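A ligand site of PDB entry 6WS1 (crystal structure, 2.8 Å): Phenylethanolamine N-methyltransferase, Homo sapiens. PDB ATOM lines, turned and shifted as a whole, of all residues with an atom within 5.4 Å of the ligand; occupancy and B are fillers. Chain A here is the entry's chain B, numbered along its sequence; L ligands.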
ATOM      1  N   VAL A  35      15.935  27.726   9.503  1.00  0.00           N
ATOM      2  CA  VAL A  35      15.955  28.176  10.890  1.00  0.00           C
ATOM      3  C   VAL A  35      17.382  28.471  11.325  1.00  0.00           C
ATOM      4  O   VAL A  35      17.647  29.493  11.965  1.00  0.00           O
ATOM      5  CB  VAL A  35      15.229  27.163  11.798  1.00  0.00           C
ATOM      6  CG1 VAL A  35      13.952  26.692  11.118  1.00  0.00           C
ATOM      7  CG2 VAL A  35      16.111  25.982  12.179  1.00  0.00           C
ATOM      8  N   TYR A  39      18.396  32.025  12.955  1.00  0.00           N
ATOM      9  CA  TYR A  39      18.938  32.114  14.300  1.00  0.00           C
ATOM     10  C   TYR A  39      20.347  32.678  14.306  1.00  0.00           C
ATOM     11  O   TYR A  39      20.875  32.946  15.391  1.00  0.00           O
ATOM     12  CB  TYR A  39      18.891  30.738  14.978  1.00  0.00           C
ATOM     13  CG  TYR A  39      17.705  30.596  15.894  1.00  0.00           C
ATOM     14  CD1 TYR A  39      17.653  31.303  17.105  1.00  0.00           C
ATOM     15  CD2 TYR A  39      16.629  29.774  15.565  1.00  0.00           C
ATOM     16  CE1 TYR A  39      16.556  31.206  17.966  1.00  0.00           C
ATOM     17  CE2 TYR A  39      15.525  29.667  16.420  1.00  0.00           C
ATOM     18  CZ  TYR A  39      15.496  30.382  17.604  1.00  0.00           C
ATOM     19  OH  TYR A  39      14.414  30.288  18.441  1.00  0.00           O
ATOM     20  N   PHE A  42      20.302  36.008  15.908  1.00  0.00           N
ATOM     21  CA  PHE A  42      19.639  35.898  17.210  1.00  0.00           C
ATOM     22  C   PHE A  42      20.177  36.889  18.218  1.00  0.00           C
ATOM     23  O   PHE A  42      21.380  37.193  18.264  1.00  0.00           O
ATOM     24  CB  PHE A  42      19.758  34.495  17.781  1.00  0.00           C
ATOM     25  CG  PHE A  42      18.916  34.274  19.013  1.00  0.00           C
ATOM     26  CD1 PHE A  42      17.532  34.469  18.969  1.00  0.00           C
ATOM     27  CD2 PHE A  42      19.499  33.913  20.229  1.00  0.00           C
ATOM     28  CE1 PHE A  42      16.752  34.290  20.102  1.00  0.00           C
ATOM     29  CE2 PHE A  42      18.726  33.727  21.365  1.00  0.00           C
ATOM     30  CZ  PHE A  42      17.349  33.919  21.300  1.00  0.00           C
ATOM     31  N   TYR A  47      16.542  39.062  23.581  1.00  0.00           N
ATOM     32  CA  TYR A  47      15.514  38.041  23.759  1.00  0.00           C
ATOM     33  C   TYR A  47      15.025  37.992  25.189  1.00  0.00           C
ATOM     34  O   TYR A  47      13.824  37.832  25.441  1.00  0.00           O
ATOM     35  CB  TYR A  47      16.067  36.678  23.329  1.00  0.00           C
ATOM     36  CG  TYR A  47      15.219  35.519  23.759  1.00  0.00           C
ATOM     37  CD1 TYR A  47      13.943  35.346  23.242  1.00  0.00           C
ATOM     38  CD2 TYR A  47      15.680  34.602  24.695  1.00  0.00           C
ATOM     39  CE1 TYR A  47      13.145  34.289  23.632  1.00  0.00           C
ATOM     40  CE2 TYR A  47      14.895  33.542  25.110  1.00  0.00           C
ATOM     41  CZ  TYR A  47      13.620  33.389  24.570  1.00  0.00           C
ATOM     42  OH  TYR A  47      12.829  32.326  24.964  1.00  0.00           O
ATOM     43  N   ASN A  51      11.199  39.008  26.716  1.00  0.00           N
ATOM     44  CA  ASN A  51      10.389  37.873  27.123  1.00  0.00           C
ATOM     45  C   ASN A  51      10.417  37.567  28.605  1.00  0.00           C
ATOM     46  O   ASN A  51       9.447  37.029  29.131  1.00  0.00           O
ATOM     47  CB  ASN A  51      10.804  36.598  26.377  1.00  0.00           C
ATOM     48  CG  ASN A  51      10.458  36.649  24.897  1.00  0.00           C
ATOM     49  OD1 ASN A  51      11.349  36.616  24.065  1.00  0.00           O
ATOM     50  ND2 ASN A  51       9.171  36.722  24.580  1.00  0.00           N
ATOM     51  N   TYR A  52      11.488  37.908  29.314  1.00  0.00           N
ATOM     52  CA  TYR A  52      11.586  37.506  30.710  1.00  0.00           C
ATOM     53  C   TYR A  52      11.777  38.642  31.706  1.00  0.00           C
ATOM     54  O   TYR A  52      11.547  38.437  32.895  1.00  0.00           O
ATOM     55  CB  TYR A  52      12.697  36.449  30.864  1.00  0.00           C
ATOM     56  CG  TYR A  52      12.317  35.163  30.143  1.00  0.00           C
ATOM     57  CD1 TYR A  52      11.467  34.237  30.736  1.00  0.00           C
ATOM     58  CD2 TYR A  52      12.770  34.906  28.857  1.00  0.00           C
ATOM     59  CE1 TYR A  52      11.104  33.068  30.090  1.00  0.00           C
ATOM     60  CE2 TYR A  52      12.414  33.734  28.191  1.00  0.00           C
ATOM     61  CZ  TYR A  52      11.570  32.810  28.804  1.00  0.00           C
ATOM     62  OH  TYR A  52      11.207  31.632  28.141  1.00  0.00           O
ATOM     63  N   VAL A  65       1.656  33.501  32.816  1.00  0.00           N
ATOM     64  CA  VAL A  65       2.305  32.408  32.116  1.00  0.00           C
ATOM     65  C   VAL A  65       3.641  32.019  32.742  1.00  0.00           C
ATOM     66  O   VAL A  65       4.017  30.839  32.709  1.00  0.00           O
ATOM     67  CB  VAL A  65       2.451  32.794  30.631  1.00  0.00           C
ATOM     68  CG1 VAL A  65       3.036  34.209  30.492  1.00  0.00           C
ATOM     69  CG2 VAL A  65       3.261  31.733  29.828  1.00  0.00           C
ATOM     70  N   LYS A  69       4.133  27.976  34.003  1.00  0.00           N
ATOM     71  CA  LYS A  69       5.258  27.092  33.687  1.00  0.00           C
ATOM     72  C   LYS A  69       5.968  26.630  34.956  1.00  0.00           C
ATOM     73  O   LYS A  69       6.285  25.448  35.115  1.00  0.00           O
ATOM     74  CB  LYS A  69       6.260  27.798  32.761  1.00  0.00           C
ATOM     75  CG  LYS A  69       5.680  28.584  31.631  1.00  0.00           C
ATOM     76  CD  LYS A  69       6.759  28.897  30.615  1.00  0.00           C
ATOM     77  CE  LYS A  69       7.445  30.208  30.834  1.00  0.00           C
ATOM     78  NZ  LYS A  69       8.536  30.360  29.832  1.00  0.00           N
ATOM     79  N   GLY A  91      18.156  22.467  24.401  1.00  0.00           N
ATOM     80  CA  GLY A  91      17.903  23.797  23.887  1.00  0.00           C
ATOM     81  C   GLY A  91      17.522  24.771  25.000  1.00  0.00           C
ATOM     82  O   GLY A  91      16.405  25.292  25.041  1.00  0.00           O
ATOM     83  N   SER A  92      18.465  25.000  25.910  1.00  0.00           N
ATOM     84  CA  SER A  92      18.196  25.849  27.056  1.00  0.00           C
ATOM     85  C   SER A  92      18.029  27.293  26.653  1.00  0.00           C
ATOM     86  O   SER A  92      17.337  28.064  27.338  1.00  0.00           O
ATOM     87  CB  SER A  92      19.330  25.721  28.072  1.00  0.00           C
ATOM     88  OG  SER A  92      19.754  24.362  28.211  1.00  0.00           O
ATOM     89  N   GLY A  93      18.627  27.698  25.548  1.00  0.00           N
ATOM     90  CA  GLY A  93      18.604  29.092  25.207  1.00  0.00           C
ATOM     91  C   GLY A  93      19.504  29.785  26.194  1.00  0.00           C
ATOM     92  O   GLY A  93      20.498  29.221  26.645  1.00  0.00           O
ATOM     93  N   PRO A  94      19.194  31.003  26.545  1.00  0.00           N
ATOM     94  CA  PRO A  94      19.969  31.663  27.591  1.00  0.00           C
ATOM     95  C   PRO A  94      19.177  31.798  28.889  1.00  0.00           C
ATOM     96  O   PRO A  94      19.180  32.849  29.533  1.00  0.00           O
ATOM     97  CB  PRO A  94      20.275  33.026  26.969  1.00  0.00           C
ATOM     98  CG  PRO A  94      18.974  33.327  26.255  1.00  0.00           C
ATOM     99  CD  PRO A  94      18.374  31.981  25.808  1.00  0.00           C
ATOM    100  N   THR A  95      18.457  30.740  29.271  1.00  0.00           N
ATOM    101  CA  THR A  95      17.532  30.777  30.403  1.00  0.00           C
ATOM    102  C   THR A  95      17.746  29.562  31.295  1.00  0.00           C
ATOM    103  O   THR A  95      18.387  28.586  30.918  1.00  0.00           O
ATOM    104  CB  THR A  95      16.066  30.820  29.941  1.00  0.00           C
ATOM    105  OG1 THR A  95      15.654  29.496  29.576  1.00  0.00           O
ATOM    106  CG2 THR A  95      15.873  31.780  28.752  1.00  0.00           C
ATOM    107  N   TYR A  97      15.093  29.226  34.329  1.00  0.00           N
ATOM    108  CA  TYR A  97      13.853  29.022  35.085  1.00  0.00           C
ATOM    109  C   TYR A  97      13.382  27.577  35.005  1.00  0.00           C
ATOM    110  O   TYR A  97      12.852  27.023  35.985  1.00  0.00           O
ATOM    111  CB  TYR A  97      12.745  29.952  34.569  1.00  0.00           C
ATOM    112  CG  TYR A  97      12.264  29.618  33.159  1.00  0.00           C
ATOM    113  CD1 TYR A  97      12.930  30.099  32.039  1.00  0.00           C
ATOM    114  CD2 TYR A  97      11.149  28.830  32.970  1.00  0.00           C
ATOM    115  CE1 TYR A  97      12.494  29.795  30.772  1.00  0.00           C
ATOM    116  CE2 TYR A  97      10.704  28.503  31.703  1.00  0.00           C
ATOM    117  CZ  TYR A  97      11.377  28.986  30.604  1.00  0.00           C
ATOM    118  OH  TYR A  97      10.911  28.663  29.357  1.00  0.00           O
ATOM    119  N   GLN A  98      13.584  26.956  33.843  1.00  0.00           N
ATOM    120  CA  GLN A  98      13.159  25.595  33.609  1.00  0.00           C
ATOM    121  C   GLN A  98      13.946  24.582  34.431  1.00  0.00           C
ATOM    122  O   GLN A  98      13.524  23.425  34.520  1.00  0.00           O
ATOM    123  CB  GLN A  98      13.257  25.287  32.095  1.00  0.00           C
ATOM    124  CG  GLN A  98      14.688  25.065  31.514  1.00  0.00           C
ATOM    125  CD  GLN A  98      15.279  26.345  30.940  1.00  0.00           C
ATOM    126  OE1 GLN A  98      14.836  27.454  31.310  1.00  0.00           O
ATOM    127  NE2 GLN A  98      16.280  26.215  30.058  1.00  0.00           N
ATOM    128  N   ASP A 113      22.750  24.510  24.056  1.00  0.00           N
ATOM    129  CA  ASP A 113      22.125  25.309  23.009  1.00  0.00           C
ATOM    130  C   ASP A 113      22.919  25.203  21.707  1.00  0.00           C
ATOM    131  O   ASP A 113      24.043  24.693  21.673  1.00  0.00           O
ATOM    132  CB  ASP A 113      21.968  26.772  23.395  1.00  0.00           C
ATOM    133  CG  ASP A 113      21.038  27.500  22.446  1.00  0.00           C
ATOM    134  OD1 ASP A 113      19.807  27.431  22.640  1.00  0.00           O
ATOM    135  OD2 ASP A 113      21.555  28.115  21.491  1.00  0.00           O
ATOM    136  N   PHE A 114      22.280  25.677  20.613  1.00  0.00           N
ATOM    137  CA  PHE A 114      22.837  25.612  19.264  1.00  0.00           C
ATOM    138  C   PHE A 114      23.779  26.788  18.973  1.00  0.00           C
ATOM    139  O   PHE A 114      24.692  26.647  18.151  1.00  0.00           O
ATOM    140  CB  PHE A 114      21.703  25.579  18.228  1.00  0.00           C
ATOM    141  CG  PHE A 114      22.177  25.485  16.780  1.00  0.00           C
ATOM    142  CD1 PHE A 114      23.228  24.635  16.412  1.00  0.00           C
ATOM    143  CD2 PHE A 114      21.592  26.275  15.784  1.00  0.00           C
ATOM    144  CE1 PHE A 114      23.663  24.574  15.104  1.00  0.00           C
ATOM    145  CE2 PHE A 114      22.042  26.214  14.476  1.00  0.00           C
ATOM    146  CZ  PHE A 114      23.076  25.358  14.155  1.00  0.00           C
ATOM    147  N   LEU A 115      23.593  27.906  19.645  1.00  0.00           N
ATOM    148  CA  LEU A 115      24.364  29.113  19.391  1.00  0.00           C
ATOM    149  C   LEU A 115      25.392  29.350  20.501  1.00  0.00           C
ATOM    150  O   LEU A 115      25.034  29.433  21.676  1.00  0.00           O
ATOM    151  CB  LEU A 115      23.428  30.318  19.300  1.00  0.00           C
ATOM    152  CG  LEU A 115      22.344  30.258  18.234  1.00  0.00           C
ATOM    153  CD1 LEU A 115      21.221  31.202  18.576  1.00  0.00           C
ATOM    154  CD2 LEU A 115      22.950  30.621  16.892  1.00  0.00           C
ATOM    155  N   ASN A 118      24.721  32.064  22.945  1.00  0.00           N
ATOM    156  CA  ASN A 118      23.781  31.749  24.010  1.00  0.00           C
ATOM    157  C   ASN A 118      24.439  30.935  25.110  1.00  0.00           C
ATOM    158  O   ASN A 118      24.202  31.179  26.306  1.00  0.00           O
ATOM    159  CB  ASN A 118      22.579  30.999  23.429  1.00  0.00           C
ATOM    160  CG  ASN A 118      21.385  31.916  23.221  1.00  0.00           C
ATOM    161  OD1 ASN A 118      21.418  33.081  23.627  1.00  0.00           O
ATOM    162  ND2 ASN A 118      20.345  31.405  22.588  1.00  0.00           N
ATOM    163  N   ILE A 169      24.326  21.776  20.807  1.00  0.00           N
ATOM    164  CA  ILE A 169      23.229  20.849  20.520  1.00  0.00           C
ATOM    165  C   ILE A 169      22.671  21.125  19.124  1.00  0.00           C
ATOM    166  O   ILE A 169      22.627  22.273  18.672  1.00  0.00           O
ATOM    167  CB  ILE A 169      22.127  20.984  21.600  1.00  0.00           C
ATOM    168  CG1 ILE A 169      21.042  19.951  21.434  1.00  0.00           C
ATOM    169  CG2 ILE A 169      21.460  22.331  21.530  1.00  0.00           C
ATOM    170  CD1 ILE A 169      21.588  18.621  21.223  1.00  0.00           C
ATOM    171  N   ASP A 170      22.273  20.059  18.425  1.00  0.00           N
ATOM    172  CA  ASP A 170      21.479  20.139  17.192  1.00  0.00           C
ATOM    173  C   ASP A 170      20.438  19.024  17.215  1.00  0.00           C
ATOM    174  O   ASP A 170      20.770  17.849  17.045  1.00  0.00           O
ATOM    175  CB  ASP A 170      22.342  20.031  15.926  1.00  0.00           C
ATOM    176  CG  ASP A 170      21.586  20.431  14.654  1.00  0.00           C
ATOM    177  OD1 ASP A 170      20.332  20.432  14.654  1.00  0.00           O
ATOM    178  OD2 ASP A 170      22.253  20.726  13.639  1.00  0.00           O
ATOM    179  N   VAL A 171      19.167  19.399  17.383  1.00  0.00           N
ATOM    180  CA  VAL A 171      18.112  18.395  17.529  1.00  0.00           C
ATOM    181  C   VAL A 171      17.857  17.589  16.252  1.00  0.00           C
ATOM    182  O   VAL A 171      17.262  16.506  16.322  1.00  0.00           O
ATOM    183  CB  VAL A 171      16.807  19.064  18.007  1.00  0.00           C
ATOM    184  CG1 VAL A 171      16.858  19.245  19.510  1.00  0.00           C
ATOM    185  CG2 VAL A 171      16.583  20.403  17.310  1.00  0.00           C
ATOM    186  N   HIS A 172      18.270  18.085  15.097  1.00  0.00           N
ATOM    187  CA  HIS A 172      17.957  17.412  13.840  1.00  0.00           C
ATOM    188  C   HIS A 172      19.017  16.407  13.417  1.00  0.00           C
ATOM    189  O   HIS A 172      18.842  15.733  12.410  1.00  0.00           O
ATOM    190  CB  HIS A 172      17.743  18.451  12.757  1.00  0.00           C
ATOM    191  CG  HIS A 172      16.651  19.427  13.071  1.00  0.00           C
ATOM    192  ND1 HIS A 172      15.341  19.040  13.269  1.00  0.00           N
ATOM    193  CD2 HIS A 172      16.669  20.784  13.211  1.00  0.00           C
ATOM    194  CE1 HIS A 172      14.603  20.114  13.528  1.00  0.00           C
ATOM    195  NE2 HIS A 172      15.387  21.178  13.493  1.00  0.00           N
ATOM    196  N   ALA A 193      12.319  23.429  26.998  1.00  0.00           N
ATOM    197  CA  ALA A 193      11.288  24.438  26.915  1.00  0.00           C
ATOM    198  C   ALA A 193      11.402  25.177  25.586  1.00  0.00           C
ATOM    199  O   ALA A 193      12.449  25.760  25.285  1.00  0.00           O
ATOM    200  CB  ALA A 193      11.385  25.407  28.084  1.00  0.00           C
ATOM    201  N   PHE A 194      10.321  25.146  24.798  1.00  0.00           N
ATOM    202  CA  PHE A 194      10.191  25.900  23.558  1.00  0.00           C
ATOM    203  C   PHE A 194      11.366  25.638  22.612  1.00  0.00           C
ATOM    204  O   PHE A 194      12.000  26.556  22.098  1.00  0.00           O
ATOM    205  CB  PHE A 194      10.054  27.384  23.832  1.00  0.00           C
ATOM    206  CG  PHE A 194       8.926  27.724  24.750  1.00  0.00           C
ATOM    207  CD1 PHE A 194       7.625  27.459  24.391  1.00  0.00           C
ATOM    208  CD2 PHE A 194       9.180  28.322  25.977  1.00  0.00           C
ATOM    209  CE1 PHE A 194       6.578  27.791  25.226  1.00  0.00           C
ATOM    210  CE2 PHE A 194       8.133  28.646  26.826  1.00  0.00           C
ATOM    211  CZ  PHE A 194       6.831  28.371  26.450  1.00  0.00           C
ATOM    212  N   CYS A 195      11.673  24.363  22.414  1.00  0.00           N
ATOM    213  CA  CYS A 195      12.662  24.023  21.414  1.00  0.00           C
ATOM    214  C   CYS A 195      11.995  23.485  20.139  1.00  0.00           C
ATOM    215  O   CYS A 195      11.860  24.193  19.136  1.00  0.00           O
ATOM    216  CB  CYS A 195      13.644  23.010  21.981  1.00  0.00           C
ATOM    217  SG  CYS A 195      15.195  22.957  21.092  1.00  0.00           S
ATOM    218  N   ALA A 198       9.656  25.062  17.802  1.00  0.00           N
ATOM    219  CA  ALA A 198      10.195  26.372  17.469  1.00  0.00           C
ATOM    220  C   ALA A 198      11.407  26.319  16.563  1.00  0.00           C
ATOM    221  O   ALA A 198      11.807  27.359  16.039  1.00  0.00           O
ATOM    222  CB  ALA A 198      10.547  27.131  18.760  1.00  0.00           C
ATOM    223  N   VAL A 199      11.996  25.138  16.355  1.00  0.00           N
ATOM    224  CA  VAL A 199      13.138  24.980  15.468  1.00  0.00           C
ATOM    225  C   VAL A 199      12.867  23.901  14.419  1.00  0.00           C
ATOM    226  O   VAL A 199      13.807  23.339  13.835  1.00  0.00           O
ATOM    227  CB  VAL A 199      14.414  24.677  16.284  1.00  0.00           C
ATOM    228  CG1 VAL A 199      14.567  25.707  17.378  1.00  0.00           C
ATOM    229  CG2 VAL A 199      14.361  23.266  16.879  1.00  0.00           C
ATOM    230  N   ALA A 228       5.087  25.918  22.462  1.00  0.00           N
ATOM    231  CA  ALA A 228       4.039  26.738  21.880  1.00  0.00           C
ATOM    232  C   ALA A 228       2.953  25.867  21.250  1.00  0.00           C
ATOM    233  O   ALA A 228       3.171  24.695  20.930  1.00  0.00           O
ATOM    234  CB  ALA A 228       4.634  27.705  20.847  1.00  0.00           C
ATOM    235  N   GLU A 231       1.384  27.592  16.796  1.00  0.00           N
ATOM    236  CA  GLU A 231       2.302  28.667  16.444  1.00  0.00           C
ATOM    237  C   GLU A 231       2.986  28.344  15.138  1.00  0.00           C
ATOM    238  O   GLU A 231       3.620  27.296  15.010  1.00  0.00           O
ATOM    239  CB  GLU A 231       3.372  28.867  17.517  1.00  0.00           C
ATOM    240  CG  GLU A 231       4.519  29.705  16.997  1.00  0.00           C
ATOM    241  CD  GLU A 231       5.805  29.576  17.781  1.00  0.00           C
ATOM    242  OE1 GLU A 231       6.224  30.619  18.312  1.00  0.00           O
ATOM    243  OE2 GLU A 231       6.401  28.470  17.816  1.00  0.00           O
ATOM    244  N   TYR A 234       7.302  33.211  14.102  1.00  0.00           N
ATOM    245  CA  TYR A 234       7.752  34.159  15.108  1.00  0.00           C
ATOM    246  C   TYR A 234       9.065  34.788  14.619  1.00  0.00           C
ATOM    247  O   TYR A 234       9.658  34.317  13.635  1.00  0.00           O
ATOM    248  CB  TYR A 234       7.895  33.512  16.495  1.00  0.00           C
ATOM    249  CG  TYR A 234       9.004  32.489  16.576  1.00  0.00           C
ATOM    250  CD1 TYR A 234       8.792  31.166  16.180  1.00  0.00           C
ATOM    251  CD2 TYR A 234      10.271  32.841  17.024  1.00  0.00           C
ATOM    252  CE1 TYR A 234       9.808  30.240  16.220  1.00  0.00           C
ATOM    253  CE2 TYR A 234      11.286  31.920  17.073  1.00  0.00           C
ATOM    254  CZ  TYR A 234      11.055  30.617  16.667  1.00  0.00           C
ATOM    255  OH  TYR A 234      12.085  29.691  16.708  1.00  0.00           O
ATOM    256  N   MET A 270      -3.344  31.346  25.881  1.00  0.00           N
ATOM    257  CA  MET A 270      -2.627  32.615  25.819  1.00  0.00           C
ATOM    258  C   MET A 270      -3.619  33.780  25.848  1.00  0.00           C
ATOM    259  O   MET A 270      -4.339  33.991  24.864  1.00  0.00           O
ATOM    260  CB  MET A 270      -1.756  32.668  24.561  1.00  0.00           C
ATOM    261  CG  MET A 270      -0.723  33.791  24.568  1.00  0.00           C
ATOM    262  SD  MET A 270       0.222  33.879  26.122  1.00  0.00           S
ATOM    263  CE  MET A 270       1.649  32.872  25.717  1.00  0.00           C
ATOM    264  N   ASP A 279       4.377  36.864  17.128  1.00  0.00           N
ATOM    265  CA  ASP A 279       4.101  35.443  16.983  1.00  0.00           C
ATOM    266  C   ASP A 279       2.619  35.286  16.656  1.00  0.00           C
ATOM    267  O   ASP A 279       1.842  36.250  16.724  1.00  0.00           O
ATOM    268  CB  ASP A 279       4.483  34.661  18.265  1.00  0.00           C
ATOM    269  CG  ASP A 279       3.943  35.300  19.557  1.00  0.00           C
ATOM    270  OD1 ASP A 279       2.885  35.973  19.544  1.00  0.00           O
ATOM    271  OD2 ASP A 279       4.606  35.142  20.603  1.00  0.00           O
ATOM    272  N   VAL A 281       1.259  32.725  18.511  1.00  0.00           N
ATOM    273  CA  VAL A 281       1.151  31.737  19.585  1.00  0.00           C
ATOM    274  C   VAL A 281      -0.210  31.861  20.250  1.00  0.00           C
ATOM    275  O   VAL A 281      -0.545  32.901  20.826  1.00  0.00           O
ATOM    276  CB  VAL A 281       2.279  31.919  20.601  1.00  0.00           C
ATOM    277  CG1 VAL A 281       2.043  31.035  21.799  1.00  0.00           C
ATOM    278  CG2 VAL A 281       3.630  31.604  19.965  1.00  0.00           C
HETATM  279  C1  LIG L   1      13.358  29.293  27.013  1.00  0.00           C
HETATM  280  N1  LIG L   1      14.702  27.438  26.242  1.00  0.00           N
HETATM  281  O1  LIG L   1      12.986  30.492  26.990  1.00  0.00           O
HETATM  282  N2  LIG L   1      18.970  22.441  17.524  1.00  0.00           N
HETATM  283  O2  LIG L   1      12.768  28.383  27.658  1.00  0.00           O
HETATM  284  C2  LIG L   1      18.999  22.709  18.836  1.00  0.00           C
HETATM  285  C3  LIG L   1      18.334  24.896  18.496  1.00  0.00           C
HETATM  286  C4  LIG L   1      18.288  24.655  17.125  1.00  0.00           C
HETATM  287  C5  LIG L   1      18.616  23.398  16.637  1.00  0.00           C
HETATM  288  C6  LIG L   1      17.729  26.704  17.497  1.00  0.00           C
HETATM  289  C7  LIG L   1      13.742  30.394  22.058  1.00  0.00           C
HETATM  290  C8  LIG L   1      12.472  29.913  21.372  1.00  0.00           C
HETATM  291  C9  LIG L   1      11.212  30.199  22.181  1.00  0.00           C
HETATM  292  C10 LIG L   1      14.590  28.914  26.251  1.00  0.00           C
HETATM  293  C11 LIG L   1      14.531  29.509  24.835  1.00  0.00           C
HETATM  294  C12 LIG L   1      14.102  28.593  23.678  1.00  0.00           C
HETATM  295  N3  LIG L   1      14.605  29.256  22.440  1.00  0.00           N
HETATM  296  C13 LIG L   1      17.893  26.861  20.001  1.00  0.00           C
HETATM  297  C14 LIG L   1      10.392  31.349  21.626  1.00  0.00           C
HETATM  298  C15 LIG L   1       9.663  30.964  20.328  1.00  0.00           C
HETATM  299  C16 LIG L   1       7.407  31.202  21.155  1.00  0.00           C
HETATM  300  C17 LIG L   1       8.030  31.077  22.543  1.00  0.00           C
HETATM  301  C18 LIG L   1       9.364  31.791  22.663  1.00  0.00           C
HETATM  302  C19 LIG L   1       9.887  31.523  24.054  1.00  0.00           C
HETATM  303  C20 LIG L   1      18.012  28.349  19.739  1.00  0.00           C
HETATM  304  C21 LIG L   1       9.087  31.830  25.062  1.00  0.00           C
HETATM  305  C22 LIG L   1       7.621  31.813  24.855  1.00  0.00           C
HETATM  306  C23 LIG L   1       7.154  31.733  23.586  1.00  0.00           C
HETATM  307  C24 LIG L   1      17.251  28.978  20.887  1.00  0.00           C
HETATM  308  C25 LIG L   1      16.292  27.885  21.338  1.00  0.00           C
HETATM  309  C26 LIG L   1      14.827  28.325  21.313  1.00  0.00           C
HETATM  310  N4  LIG L   1       8.416  31.755  20.240  1.00  0.00           N
HETATM  311  N5  LIG L   1      18.690  23.912  19.329  1.00  0.00           N
HETATM  312  N6  LIG L   1      18.567  23.129  15.303  1.00  0.00           N
HETATM  313  N7  LIG L   1      17.909  25.787  16.531  1.00  0.00           N
HETATM  314  N8  LIG L   1      17.984  26.160  18.699  1.00  0.00           N
HETATM  315  O3  LIG L   1      19.374  28.764  19.697  1.00  0.00           O
HETATM  316  O4  LIG L   1      18.159  29.339  21.942  1.00  0.00           O
HETATM  317  O5  LIG L   1      16.575  26.738  20.513  1.00  0.00           O
HETATM  318 CL1  LIG L   1       6.616  31.940  26.311  1.00  0.00          CL
HETATM  319 CL2  LIG L   1       5.624  32.435  23.033  1.00  0.00          CL
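The side-chain hydroxyl of Tyr 97 sits at hydrogen-bond distance from the side-chain hydroxyl of Tyr 52, 3.2 Å away.
The side-chain hydroxyl (OH) of Tyr 52 lies within hydrogen-bond range of the side-chain amino group (NZ) of Lys 69, 3.4 Å away.
The side-chain amino group of Lys 69 lies within hydrogen-bond range of the side-chain hydroxyl of Tyr 97 (3.0 Å).
The side-chain carboxylate (OD2) of Asp 113 sits at hydrogen-bond distance from the backbone NH (N) of Leu 115.
OD1 of Asp 113 is in hydrogen-bond range of N of Gly 93, at 3.1 Å.
The backbone carbonyl oxygen (O) of Asp 113 lies within hydrogen-bond range of the backbone NH (N) of Ile 169, 3.1 Å away.
The backbone carbonyl oxygen (O) of Val 199 lies within hydrogen-bond range of a ring nitrogen (NE2) of His 172 (2.7 Å).
The side-chain hydroxyl (OH) of Tyr 234 is in hydrogen-bond range of the backbone carbonyl oxygen (O) of Ala 198, at 2.4 Å.
The side-chain hydroxyl (OH) of Tyr 52 sits at hydrogen-bond distance from an oxygen (O1) of the ligand (2.4 Å).
The side-chain hydroxyl (OH) of Tyr 97 lies within hydrogen-bond range of an oxygen (O2) of the ligand, 2.5 Å away.
The side-chain carboxylate of Asp 113 is in hydrogen-bond range of an oxygen (O4) of the ligand, 2.6 Å away.
O1 of the ligand sits at hydrogen-bond distance from OH of Tyr 47 (2.7 Å).
A nitrogen (N1) of the ligand is in hydrogen-bond range of the backbone carbonyl oxygen (O) of Ser 92 (2.9 Å).
N1 of the ligand lies within hydrogen-bond range of O of Ala 193, 3.0 Å away.
The backbone carbonyl oxygen of Gly 91 lies within hydrogen-bond range of a nitrogen (N1) of the ligand.
N of Val 171 is in hydrogen-bond range of N2 of the ligand (3.1 Å).
An oxygen (O4) of the ligand is in hydrogen-bond range of the side-chain amide nitrogen of Asn 118, at 3.1 Å.
The side-chain carboxylate of Glu 231 lies within salt-bridge range of a nitrogen (N4) of the ligand (3.1 Å).
The side-chain carboxylate (OD1) of Asp 170 sits at hydrogen-bond distance from a nitrogen (N6) of the ligand (3.3 Å).
Residues that only touch the ligand: Tyr 39 (3.5 Å), Gly 93 (3.3 Å), Thr 95 (3.4 Å), Phe 114 (3.4 Å), Leu 115 (3.3 Å), Ile 169 (3.7 Å), His 172 (3.7 Å), Phe 194 (3.3 Å), Val 199 (3.3 Å), Tyr 234 (3.8 Å), Asp 279 (3.8 Å) and Val 281 (3.8 Å).
Hydrophobic or aromatic side chains within 4 Å of the ligand: Tyr 39, Tyr 47, Tyr 52, Tyr 97, Phe 114, Leu 115, Ile 169, Val 171, His 172, Ala 193, Phe 194, Val 199, Tyr 234 and Val 281.
Of the 34 residues printed, 23 come within 4 Å of the ligand.
The nearest printed residue that does not touch the ligand is Cys 195 (4.03 Å).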
